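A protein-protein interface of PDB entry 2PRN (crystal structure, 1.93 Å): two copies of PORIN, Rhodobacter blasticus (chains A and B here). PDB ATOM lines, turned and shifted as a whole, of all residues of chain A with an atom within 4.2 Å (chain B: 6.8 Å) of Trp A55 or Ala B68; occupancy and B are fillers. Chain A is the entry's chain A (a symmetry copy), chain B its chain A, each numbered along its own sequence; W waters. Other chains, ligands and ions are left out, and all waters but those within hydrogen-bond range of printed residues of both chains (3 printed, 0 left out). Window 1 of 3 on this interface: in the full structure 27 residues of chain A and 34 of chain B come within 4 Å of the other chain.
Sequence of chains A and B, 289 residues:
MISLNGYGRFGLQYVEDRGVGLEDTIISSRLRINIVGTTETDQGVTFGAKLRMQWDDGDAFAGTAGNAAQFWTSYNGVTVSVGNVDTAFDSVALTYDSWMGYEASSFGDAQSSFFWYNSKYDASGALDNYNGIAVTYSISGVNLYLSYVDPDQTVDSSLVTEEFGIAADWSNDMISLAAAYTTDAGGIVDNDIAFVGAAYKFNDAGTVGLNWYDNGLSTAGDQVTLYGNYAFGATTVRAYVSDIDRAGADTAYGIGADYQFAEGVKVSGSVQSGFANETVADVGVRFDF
The backbone NH (N) of Ala B68 is in hydrogen-bond range of the backbone carbonyl oxygen (O) of Ala A62 (3.3 Å).
OG1 of Thr A64 is in hydrogen-bond range of O of Asn B67, at 2.8 Å.
The backbone carbonyl oxygen (O) of Thr A64 is in hydrogen-bond range of the backbone NH (N) of Gly B66 (2.7 Å).
No position is printed for both chains.
Among the printed residues, pairs that only touch across the chains: Ser A29 with Phe B71 (3.5 Å), Arg A30 with Phe B71 (3.3 Å), Leu A31 with Leu B51 (3.9 Å), Leu A31 with Ala B69 (3.8 Å), Leu A31 with Phe B71 (3.9 Å), Trp A55 with Ala B68 (3.6 Å), Trp A55 with Ala B69 (3.6 Å), Trp A55 with Phe B71 (3.9 Å), Asp A59 with Asp B128 (3.7 Å), Ala A62 with Asn B67 (3.5 Å), Ala A62 with Tyr B121 (3.4 Å), Ala A62 with Leu B127 (3.6 Å), Ala A62 with Asp B128 (3.6 Å), Gly A63 with Gly B66 (3.2 Å), Gly A63 with Asn B67 (3.9 Å), Gly A63 with Tyr B121 (3.8 Å) and Thr A64 with Leu B51 (3.6 Å).
OD2 of Asp A56 is in salt-bridge range of NE of Arg A30, 2.8 Å away.
N of Arg B52 sits at hydrogen-bond distance from OD1 of Asn B67, at 2.9 Å.
The backbone carbonyl oxygen (O) of Ser A29 is in hydrogen-bond range of the backbone NH (N) of Asp A57 (3.2 Å).
ND2 of Asn B84 sits close to ND2 of Asn B67 (3.4 Å).
The backbone carbonyl oxygen (O) of Asn B118 is in hydrogen-bond range of the side-chain amide nitrogen (ND2) of Asn B67.
OD2 of Asp A59 lies within hydrogen-bond range of N of Asp A56 (2.8 Å).
Of the 20 printed residues of chain B, 9 touch a printed residue of chain A.
Hydrophobic or aromatic side chains of chain B within 4 Å of the printed part of chain A: Leu B51, Ala B68, Ala B69, Phe B71, Tyr B121 and Leu B127.
Along chain B the printed residues that touch a printed residue of chain A span positions 51 to 128.
Of the 11 printed residues of chain A, 8 touch a printed residue of chain B.
Hydrophobic or aromatic side chains of chain A within 4 Å of the printed part of chain B: Leu A31, Trp A55 and Ala A62.
Among the printed residues, 20 pairs touch across the chains.
Among the printed residues, no Asp or Glu carboxylate lies within 4 Å of a Lys or Arg side-chain nitrogen of the other chain.
Of the printed residues of chain B, Arg A30 touches Phe B71 (3.3 Å).
Of the printed residues of chain B, Trp A55 touches Ala B68, Ala B69 and Phe B71.
Printed residues of chain B within 4 Å of Asp A59: Asp B128 (3.7 Å).
Lys B50 touches none of the printed residues of chain A.
Arg B52 touches none of the printed residues of chain A.
Of the printed residues of chain A, Leu B127 touches Ala A62.
The nearest printed residue of chain A that does not touch Ala B68 is Gly A63 (4.6 Å).
The nearest printed residue of chain A that does not touch Tyr B121 is Thr A64 (5.5 Å).
Water W1 bridges OG of Ser A29 (2.6 Å) and OD1 of Asn B131 (3.1 Å).
Water W2 lies within hydrogen-bond range of the backbone carbonyl oxygen of Ala A62, the backbone carbonyl oxygen of Lys B120 and the backbone NH of Ala B68.
Water W3 lies within hydrogen-bond range of O of Asp A59 (2.8 Å), NE1 of Trp A55 (3.0 Å) and O of Asp B128 (3.5 Å).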
ATOM      1  N   SER A  29      13.845   8.308   6.665  1.00  0.00           N
ATOM      2  CA  SER A  29      15.147   8.897   6.989  1.00  0.00           C
ATOM      3  C   SER A  29      16.214   7.838   7.213  1.00  0.00           C
ATOM      4  O   SER A  29      15.896   6.682   7.444  1.00  0.00           O
ATOM      5  CB  SER A  29      15.021   9.818   8.197  1.00  0.00           C
ATOM      6  OG  SER A  29      14.496   9.094   9.298  1.00  0.00           O
ATOM      7  N   ARG A  30      17.480   8.226   7.129  1.00  0.00           N
ATOM      8  CA  ARG A  30      18.568   7.264   7.291  1.00  0.00           C
ATOM      9  C   ARG A  30      19.757   8.000   7.942  1.00  0.00           C
ATOM     10  O   ARG A  30      20.023   9.144   7.547  1.00  0.00           O
ATOM     11  CB  ARG A  30      19.071   6.799   5.907  1.00  0.00           C
ATOM     12  CG  ARG A  30      20.344   5.919   6.052  1.00  0.00           C
ATOM     13  CD  ARG A  30      20.723   5.427   4.664  1.00  0.00           C
ATOM     14  NE  ARG A  30      19.854   4.350   4.260  1.00  0.00           N
ATOM     15  CZ  ARG A  30      20.044   3.710   3.081  1.00  0.00           C
ATOM     16  NH1 ARG A  30      21.036   4.044   2.298  1.00  0.00           N
ATOM     17  NH2 ARG A  30      19.203   2.774   2.779  1.00  0.00           N
ATOM     18  N   LEU A  31      20.400   7.369   8.905  1.00  0.00           N
ATOM     19  CA  LEU A  31      21.648   7.926   9.416  1.00  0.00           C
ATOM     20  C   LEU A  31      22.750   6.878   9.095  1.00  0.00           C
ATOM     21  O   LEU A  31      22.584   5.718   9.519  1.00  0.00           O
ATOM     22  CB  LEU A  31      21.606   8.228  10.897  1.00  0.00           C
ATOM     23  CG  LEU A  31      22.950   8.447  11.609  1.00  0.00           C
ATOM     24  CD1 LEU A  31      23.687   9.608  10.986  1.00  0.00           C
ATOM     25  CD2 LEU A  31      22.742   8.685  13.097  1.00  0.00           C
ATOM     26  N   GLN A  54      24.410   1.886  10.658  1.00  0.00           N
ATOM     27  CA  GLN A  54      23.377   2.512   9.859  1.00  0.00           C
ATOM     28  C   GLN A  54      22.007   2.234  10.490  1.00  0.00           C
ATOM     29  O   GLN A  54      21.672   1.101  10.781  1.00  0.00           O
ATOM     30  CB  GLN A  54      23.368   1.960   8.428  1.00  0.00           C
ATOM     31  CG  GLN A  54      22.359   2.745   7.524  1.00  0.00           C
ATOM     32  CD  GLN A  54      22.529   2.210   6.120  1.00  0.00           C
ATOM     33  OE1 GLN A  54      23.635   2.271   5.529  1.00  0.00           O
ATOM     34  NE2 GLN A  54      21.499   1.637   5.526  1.00  0.00           N
ATOM     35  N   TRP A  55      21.220   3.297  10.568  1.00  0.00           N
ATOM     36  CA  TRP A  55      19.871   3.254  11.037  1.00  0.00           C
ATOM     37  C   TRP A  55      18.916   3.741   9.938  1.00  0.00           C
ATOM     38  O   TRP A  55      19.163   4.739   9.243  1.00  0.00           O
ATOM     39  CB  TRP A  55      19.724   4.143  12.302  1.00  0.00           C
ATOM     40  CG  TRP A  55      18.261   4.202  12.731  1.00  0.00           C
ATOM     41  CD1 TRP A  55      17.628   3.320  13.568  1.00  0.00           C
ATOM     42  CD2 TRP A  55      17.280   5.182  12.378  1.00  0.00           C
ATOM     43  NE1 TRP A  55      16.337   3.685  13.751  1.00  0.00           N
ATOM     44  CE2 TRP A  55      16.066   4.798  12.986  1.00  0.00           C
ATOM     45  CE3 TRP A  55      17.272   6.271  11.502  1.00  0.00           C
ATOM     46  CZ2 TRP A  55      14.884   5.512  12.853  1.00  0.00           C
ATOM     47  CZ3 TRP A  55      16.085   6.993  11.369  1.00  0.00           C
ATOM     48  CH2 TRP A  55      14.891   6.604  12.024  1.00  0.00           C
ATOM     49  N   ASP A  56      17.791   3.025   9.766  1.00  0.00           N
ATOM     50  CA  ASP A  56      16.731   3.428   8.855  1.00  0.00           C
ATOM     51  C   ASP A  56      15.388   3.484   9.580  1.00  0.00           C
ATOM     52  O   ASP A  56      15.177   2.693  10.499  1.00  0.00           O
ATOM     53  CB  ASP A  56      16.604   2.526   7.626  1.00  0.00           C
ATOM     54  CG  ASP A  56      17.808   2.627   6.695  1.00  0.00           C
ATOM     55  OD1 ASP A  56      18.797   1.868   6.850  1.00  0.00           O
ATOM     56  OD2 ASP A  56      17.739   3.419   5.765  1.00  0.00           O
ATOM     57  N   ASP A  57      14.523   4.418   9.200  1.00  0.00           N
ATOM     58  CA  ASP A  57      13.190   4.489   9.844  1.00  0.00           C
ATOM     59  C   ASP A  57      12.539   3.107   9.685  1.00  0.00           C
ATOM     60  O   ASP A  57      12.696   2.462   8.651  1.00  0.00           O
ATOM     61  CB  ASP A  57      12.332   5.603   9.245  1.00  0.00           C
ATOM     62  CG  ASP A  57      12.002   5.304   7.795  1.00  0.00           C
ATOM     63  OD1 ASP A  57      12.869   5.644   6.969  1.00  0.00           O
ATOM     64  OD2 ASP A  57      10.973   4.698   7.449  1.00  0.00           O
ATOM     65  N   ASP A  59      13.446   0.438  11.351  1.00  0.00           N
ATOM     66  CA  ASP A  59      14.321  -0.631  11.804  1.00  0.00           C
ATOM     67  C   ASP A  59      13.843  -1.249  13.125  1.00  0.00           C
ATOM     68  O   ASP A  59      13.382  -0.572  14.072  1.00  0.00           O
ATOM     69  CB  ASP A  59      15.763  -0.176  12.057  1.00  0.00           C
ATOM     70  CG  ASP A  59      16.627  -0.102  10.829  1.00  0.00           C
ATOM     71  OD1 ASP A  59      16.208  -0.609   9.807  1.00  0.00           O
ATOM     72  OD2 ASP A  59      17.742   0.479  10.916  1.00  0.00           O
ATOM     73  N   ALA A  62      14.178  -0.069  17.199  1.00  0.00           N
ATOM     74  CA  ALA A  62      14.475   1.364  17.305  1.00  0.00           C
ATOM     75  C   ALA A  62      15.893   1.535  17.829  1.00  0.00           C
ATOM     76  O   ALA A  62      16.212   2.340  18.688  1.00  0.00           O
ATOM     77  CB  ALA A  62      13.385   2.022  18.160  1.00  0.00           C
ATOM     78  N   GLY A  63      16.834   0.753  17.253  1.00  0.00           N
ATOM     79  CA  GLY A  63      18.229   0.775  17.665  1.00  0.00           C
ATOM     80  C   GLY A  63      19.154   0.636  16.446  1.00  0.00           C
ATOM     81  O   GLY A  63      18.716   0.377  15.330  1.00  0.00           O
ATOM     82  N   THR A  64      20.424   0.873  16.713  1.00  0.00           N
ATOM     83  CA  THR A  64      21.473   0.828  15.695  1.00  0.00           C
ATOM     84  C   THR A  64      22.604  -0.016  16.231  1.00  0.00           C
ATOM     85  O   THR A  64      23.004   0.110  17.416  1.00  0.00           O
ATOM     86  CB  THR A  64      21.951   2.271  15.436  1.00  0.00           C
ATOM     87  OG1 THR A  64      20.815   3.092  15.159  1.00  0.00           O
ATOM     88  CG2 THR A  64      22.920   2.402  14.262  1.00  0.00           C
ATOM     89  N   LYS B  50      22.173  12.996  15.108  1.00  0.00           N
ATOM     90  CA  LYS B  50      22.757  12.515  16.330  1.00  0.00           C
ATOM     91  C   LYS B  50      22.292  11.105  16.674  1.00  0.00           C
ATOM     92  O   LYS B  50      21.157  10.700  16.439  1.00  0.00           O
ATOM     93  CB  LYS B  50      22.563  13.492  17.438  1.00  0.00           C
ATOM     94  CG  LYS B  50      21.638  13.137  18.564  1.00  0.00           C
ATOM     95  CD  LYS B  50      21.973  13.911  19.846  1.00  0.00           C
ATOM     96  CE  LYS B  50      20.749  14.122  20.728  1.00  0.00           C
ATOM     97  NZ  LYS B  50      20.984  15.061  21.853  1.00  0.00           N
ATOM     98  N   LEU B  51      23.246  10.399  17.233  1.00  0.00           N
ATOM     99  CA  LEU B  51      23.048   9.047  17.703  1.00  0.00           C
ATOM    100  C   LEU B  51      23.547   8.992  19.153  1.00  0.00           C
ATOM    101  O   LEU B  51      24.594   9.613  19.486  1.00  0.00           O
ATOM    102  CB  LEU B  51      23.748   8.038  16.787  1.00  0.00           C
ATOM    103  CG  LEU B  51      23.374   6.563  17.016  1.00  0.00           C
ATOM    104  CD1 LEU B  51      21.990   6.284  16.476  1.00  0.00           C
ATOM    105  CD2 LEU B  51      24.381   5.636  16.337  1.00  0.00           C
ATOM    106  N   ARG B  52      22.927   8.185  19.990  1.00  0.00           N
ATOM    107  CA  ARG B  52      23.389   7.991  21.354  1.00  0.00           C
ATOM    108  C   ARG B  52      23.669   6.518  21.647  1.00  0.00           C
ATOM    109  O   ARG B  52      22.906   5.617  21.212  1.00  0.00           O
ATOM    110  CB  ARG B  52      22.319   8.489  22.372  1.00  0.00           C
ATOM    111  CG  ARG B  52      22.742   8.311  23.829  1.00  0.00           C
ATOM    112  CD  ARG B  52      21.852   9.130  24.784  1.00  0.00           C
ATOM    113  NE  ARG B  52      22.124  10.582  24.602  1.00  0.00           N
ATOM    114  CZ  ARG B  52      21.391  11.542  25.164  1.00  0.00           C
ATOM    115  NH1 ARG B  52      20.331  11.213  25.954  1.00  0.00           N
ATOM    116  NH2 ARG B  52      21.687  12.830  24.970  1.00  0.00           N
ATOM    117  N   GLY B  66      23.284   1.521  19.754  1.00  0.00           N
ATOM    118  CA  GLY B  66      22.866   2.924  19.501  1.00  0.00           C
ATOM    119  C   GLY B  66      21.315   2.947  19.549  1.00  0.00           C
ATOM    120  O   GLY B  66      20.638   1.915  19.498  1.00  0.00           O
ATOM    121  N   ASN B  67      20.769   4.155  19.653  1.00  0.00           N
ATOM    122  CA  ASN B  67      19.309   4.339  19.681  1.00  0.00           C
ATOM    123  C   ASN B  67      18.817   4.670  18.264  1.00  0.00           C
ATOM    124  O   ASN B  67      19.523   4.427  17.296  1.00  0.00           O
ATOM    125  CB  ASN B  67      18.955   5.409  20.691  1.00  0.00           C
ATOM    126  CG  ASN B  67      19.505   6.774  20.384  1.00  0.00           C
ATOM    127  OD1 ASN B  67      20.393   6.918  19.523  1.00  0.00           O
ATOM    128  ND2 ASN B  67      19.072   7.814  21.089  1.00  0.00           N
ATOM    129  N   ALA B  68      17.647   5.294  18.140  1.00  0.00           N
ATOM    130  CA  ALA B  68      17.106   5.734  16.860  1.00  0.00           C
ATOM    131  C   ALA B  68      17.554   7.179  16.651  1.00  0.00           C
ATOM    132  O   ALA B  68      17.696   7.962  17.595  1.00  0.00           O
ATOM    133  CB  ALA B  68      15.600   5.549  16.790  1.00  0.00           C
ATOM    134  N   ALA B  69      17.859   7.488  15.409  1.00  0.00           N
ATOM    135  CA  ALA B  69      18.447   8.755  15.031  1.00  0.00           C
ATOM    136  C   ALA B  69      17.520   9.969  15.132  1.00  0.00           C
ATOM    137  O   ALA B  69      16.301   9.873  15.043  1.00  0.00           O
ATOM    138  CB  ALA B  69      18.885   8.716  13.555  1.00  0.00           C
ATOM    139  N   GLN B  70      18.187  11.096  15.300  1.00  0.00           N
ATOM    140  CA  GLN B  70      17.550  12.411  15.359  1.00  0.00           C
ATOM    141  C   GLN B  70      18.222  13.285  14.288  1.00  0.00           C
ATOM    142  O   GLN B  70      19.476  13.221  14.184  1.00  0.00           O
ATOM    143  CB  GLN B  70      17.707  13.053  16.734  1.00  0.00           C
ATOM    144  CG  GLN B  70      17.109  14.469  16.779  1.00  0.00           C
ATOM    145  CD  GLN B  70      17.419  15.195  18.073  1.00  0.00           C
ATOM    146  OE1 GLN B  70      18.213  16.142  18.069  1.00  0.00           O
ATOM    147  NE2 GLN B  70      16.833  14.814  19.193  1.00  0.00           N
ATOM    148  N   PHE B  71      17.447  14.066  13.558  1.00  0.00           N
ATOM    149  CA  PHE B  71      17.973  14.921  12.519  1.00  0.00           C
ATOM    150  C   PHE B  71      17.476  16.351  12.767  1.00  0.00           C
ATOM    151  O   PHE B  71      16.362  16.530  13.271  1.00  0.00           O
ATOM    152  CB  PHE B  71      17.534  14.516  11.091  1.00  0.00           C
ATOM    153  CG  PHE B  71      17.789  13.059  10.775  1.00  0.00           C
ATOM    154  CD1 PHE B  71      16.856  12.115  11.175  1.00  0.00           C
ATOM    155  CD2 PHE B  71      18.941  12.635  10.146  1.00  0.00           C
ATOM    156  CE1 PHE B  71      17.064  10.754  10.946  1.00  0.00           C
ATOM    157  CE2 PHE B  71      19.142  11.263   9.893  1.00  0.00           C
ATOM    158  CZ  PHE B  71      18.206  10.305  10.257  1.00  0.00           C
ATOM    159  N   GLY B  83      12.342  12.764  13.713  1.00  0.00           N
ATOM    160  CA  GLY B  83      12.837  11.467  14.163  1.00  0.00           C
ATOM    161  C   GLY B  83      12.687  11.243  15.635  1.00  0.00           C
ATOM    162  O   GLY B  83      11.573  11.306  16.172  1.00  0.00           O
ATOM    163  N   ASN B  84      13.768  10.933  16.352  1.00  0.00           N
ATOM    164  CA  ASN B  84      13.725  10.743  17.822  1.00  0.00           C
ATOM    165  C   ASN B  84      14.015  12.106  18.440  1.00  0.00           C
ATOM    166  O   ASN B  84      15.119  12.497  18.790  1.00  0.00           O
ATOM    167  CB  ASN B  84      14.774   9.677  18.177  1.00  0.00           C
ATOM    168  CG  ASN B  84      14.896   9.327  19.639  1.00  0.00           C
ATOM    169  OD1 ASN B  84      14.034   9.714  20.478  1.00  0.00           O
ATOM    170  ND2 ASN B  84      15.955   8.555  19.983  1.00  0.00           N
ATOM    171  N   TYR B 117      12.833  12.173  24.512  1.00  0.00           N
ATOM    172  CA  TYR B 117      13.926  11.597  23.724  1.00  0.00           C
ATOM    173  C   TYR B 117      14.238  10.181  24.246  1.00  0.00           C
ATOM    174  O   TYR B 117      14.395   9.991  25.436  1.00  0.00           O
ATOM    175  CB  TYR B 117      15.164  12.475  23.855  1.00  0.00           C
ATOM    176  CG  TYR B 117      16.364  12.019  23.041  1.00  0.00           C
ATOM    177  CD1 TYR B 117      16.383  12.120  21.668  1.00  0.00           C
ATOM    178  CD2 TYR B 117      17.442  11.467  23.706  1.00  0.00           C
ATOM    179  CE1 TYR B 117      17.492  11.687  20.907  1.00  0.00           C
ATOM    180  CE2 TYR B 117      18.573  11.039  22.969  1.00  0.00           C
ATOM    181  CZ  TYR B 117      18.584  11.162  21.612  1.00  0.00           C
ATOM    182  OH  TYR B 117      19.684  10.736  20.900  1.00  0.00           O
ATOM    183  N   ASN B 118      14.318   9.215  23.325  1.00  0.00           N
ATOM    184  CA  ASN B 118      14.608   7.825  23.696  1.00  0.00           C
ATOM    185  C   ASN B 118      16.097   7.547  23.601  1.00  0.00           C
ATOM    186  O   ASN B 118      16.687   7.544  22.483  1.00  0.00           O
ATOM    187  CB  ASN B 118      13.849   6.851  22.782  1.00  0.00           C
ATOM    188  CG  ASN B 118      12.346   7.056  22.869  1.00  0.00           C
ATOM    189  OD1 ASN B 118      11.785   7.114  23.953  1.00  0.00           O
ATOM    190  ND2 ASN B 118      11.673   7.215  21.734  1.00  0.00           N
ATOM    191  N   SER B 119      16.745   7.373  24.743  1.00  0.00           N
ATOM    192  CA  SER B 119      18.150   7.233  24.836  1.00  0.00           C
ATOM    193  C   SER B 119      18.649   5.894  24.356  1.00  0.00           C
ATOM    194  O   SER B 119      19.841   5.803  24.041  1.00  0.00           O
ATOM    195  CB  SER B 119      18.612   7.388  26.336  1.00  0.00           C
ATOM    196  OG  SER B 119      18.696   8.777  26.555  1.00  0.00           O
ATOM    197  N   LYS B 120      17.783   4.876  24.328  1.00  0.00           N
ATOM    198  CA  LYS B 120      18.143   3.546  23.973  1.00  0.00           C
ATOM    199  C   LYS B 120      17.162   2.855  23.043  1.00  0.00           C
ATOM    200  O   LYS B 120      16.087   3.397  22.808  1.00  0.00           O
ATOM    201  CB  LYS B 120      18.170   2.673  25.257  1.00  0.00           C
ATOM    202  CG  LYS B 120      19.345   3.044  26.153  1.00  0.00           C
ATOM    203  CD  LYS B 120      19.342   2.221  27.421  1.00  0.00           C
ATOM    204  CE  LYS B 120      20.316   2.782  28.432  1.00  0.00           C
ATOM    205  NZ  LYS B 120      20.399   1.864  29.608  1.00  0.00           N
ATOM    206  N   TYR B 121      17.510   1.697  22.565  1.00  0.00           N
ATOM    207  CA  TYR B 121      16.662   0.846  21.760  1.00  0.00           C
ATOM    208  C   TYR B 121      15.523   0.382  22.695  1.00  0.00           C
ATOM    209  O   TYR B 121      15.600   0.493  23.936  1.00  0.00           O
ATOM    210  CB  TYR B 121      17.450  -0.358  21.215  1.00  0.00           C
ATOM    211  CG  TYR B 121      17.751  -1.436  22.261  1.00  0.00           C
ATOM    212  CD1 TYR B 121      18.897  -1.346  23.021  1.00  0.00           C
ATOM    213  CD2 TYR B 121      16.894  -2.515  22.504  1.00  0.00           C
ATOM    214  CE1 TYR B 121      19.215  -2.285  23.990  1.00  0.00           C
ATOM    215  CE2 TYR B 121      17.195  -3.490  23.440  1.00  0.00           C
ATOM    216  CZ  TYR B 121      18.369  -3.358  24.179  1.00  0.00           C
ATOM    217  OH  TYR B 121      18.719  -4.263  25.152  1.00  0.00           O
ATOM    218  N   LEU B 127       8.741   1.077  19.670  1.00  0.00           N
ATOM    219  CA  LEU B 127       9.187   2.317  19.028  1.00  0.00           C
ATOM    220  C   LEU B 127       9.596   2.164  17.574  1.00  0.00           C
ATOM    221  O   LEU B 127      10.068   3.149  16.982  1.00  0.00           O
ATOM    222  CB  LEU B 127      10.338   2.893  19.836  1.00  0.00           C
ATOM    223  CG  LEU B 127      10.120   3.186  21.316  1.00  0.00           C
ATOM    224  CD1 LEU B 127      11.434   3.594  21.953  1.00  0.00           C
ATOM    225  CD2 LEU B 127       9.033   4.262  21.466  1.00  0.00           C
ATOM    226  N   ASP B 128       9.390   1.061  16.906  1.00  0.00           N
ATOM    227  CA  ASP B 128       9.882   0.801  15.558  1.00  0.00           C
ATOM    228  C   ASP B 128       9.473   1.821  14.512  1.00  0.00           C
ATOM    229  O   ASP B 128      10.297   2.142  13.646  1.00  0.00           O
ATOM    230  CB  ASP B 128       9.507  -0.599  15.048  1.00  0.00           C
ATOM    231  CG  ASP B 128      10.238  -1.730  15.736  1.00  0.00           C
ATOM    232  OD1 ASP B 128      10.928  -1.549  16.771  1.00  0.00           O
ATOM    233  OD2 ASP B 128      10.127  -2.886  15.284  1.00  0.00           O
ATOM    234  N   TYR B 130       8.045   4.882  15.383  1.00  0.00           N
ATOM    235  CA  TYR B 130       7.817   6.092  16.152  1.00  0.00           C
ATOM    236  C   TYR B 130       8.564   7.225  15.465  1.00  0.00           C
ATOM    237  O   TYR B 130       9.730   7.119  15.110  1.00  0.00           O
ATOM    238  CB  TYR B 130       8.305   5.802  17.556  1.00  0.00           C
ATOM    239  CG  TYR B 130       8.481   6.927  18.534  1.00  0.00           C
ATOM    240  CD1 TYR B 130       9.507   7.855  18.367  1.00  0.00           C
ATOM    241  CD2 TYR B 130       7.620   7.025  19.624  1.00  0.00           C
ATOM    242  CE1 TYR B 130       9.693   8.861  19.294  1.00  0.00           C
ATOM    243  CE2 TYR B 130       7.797   8.038  20.560  1.00  0.00           C
ATOM    244  CZ  TYR B 130       8.843   8.942  20.399  1.00  0.00           C
ATOM    245  OH  TYR B 130       9.027   9.922  21.319  1.00  0.00           O
ATOM    246  N   ASN B 131       7.885   8.341  15.245  1.00  0.00           N
ATOM    247  CA  ASN B 131       8.505   9.485  14.580  1.00  0.00           C
ATOM    248  C   ASN B 131       7.948  10.795  15.088  1.00  0.00           C
ATOM    249  O   ASN B 131       6.738  10.942  15.261  1.00  0.00           O
ATOM    250  CB  ASN B 131       8.319   9.318  13.073  1.00  0.00           C
ATOM    251  CG  ASN B 131       9.201  10.267  12.307  1.00  0.00           C
ATOM    252  OD1 ASN B 131      10.398  10.006  12.201  1.00  0.00           O
ATOM    253  ND2 ASN B 131       8.648  11.348  11.796  1.00  0.00           N
HETATM  254  O   HOH W   1      11.960   9.003   9.760  1.00  0.00           O
HETATM  255  O   HOH W   2      15.507   4.595  20.202  1.00  0.00           O
HETATM  256  O   HOH W   3      13.747   2.208  14.222  1.00  0.00           O
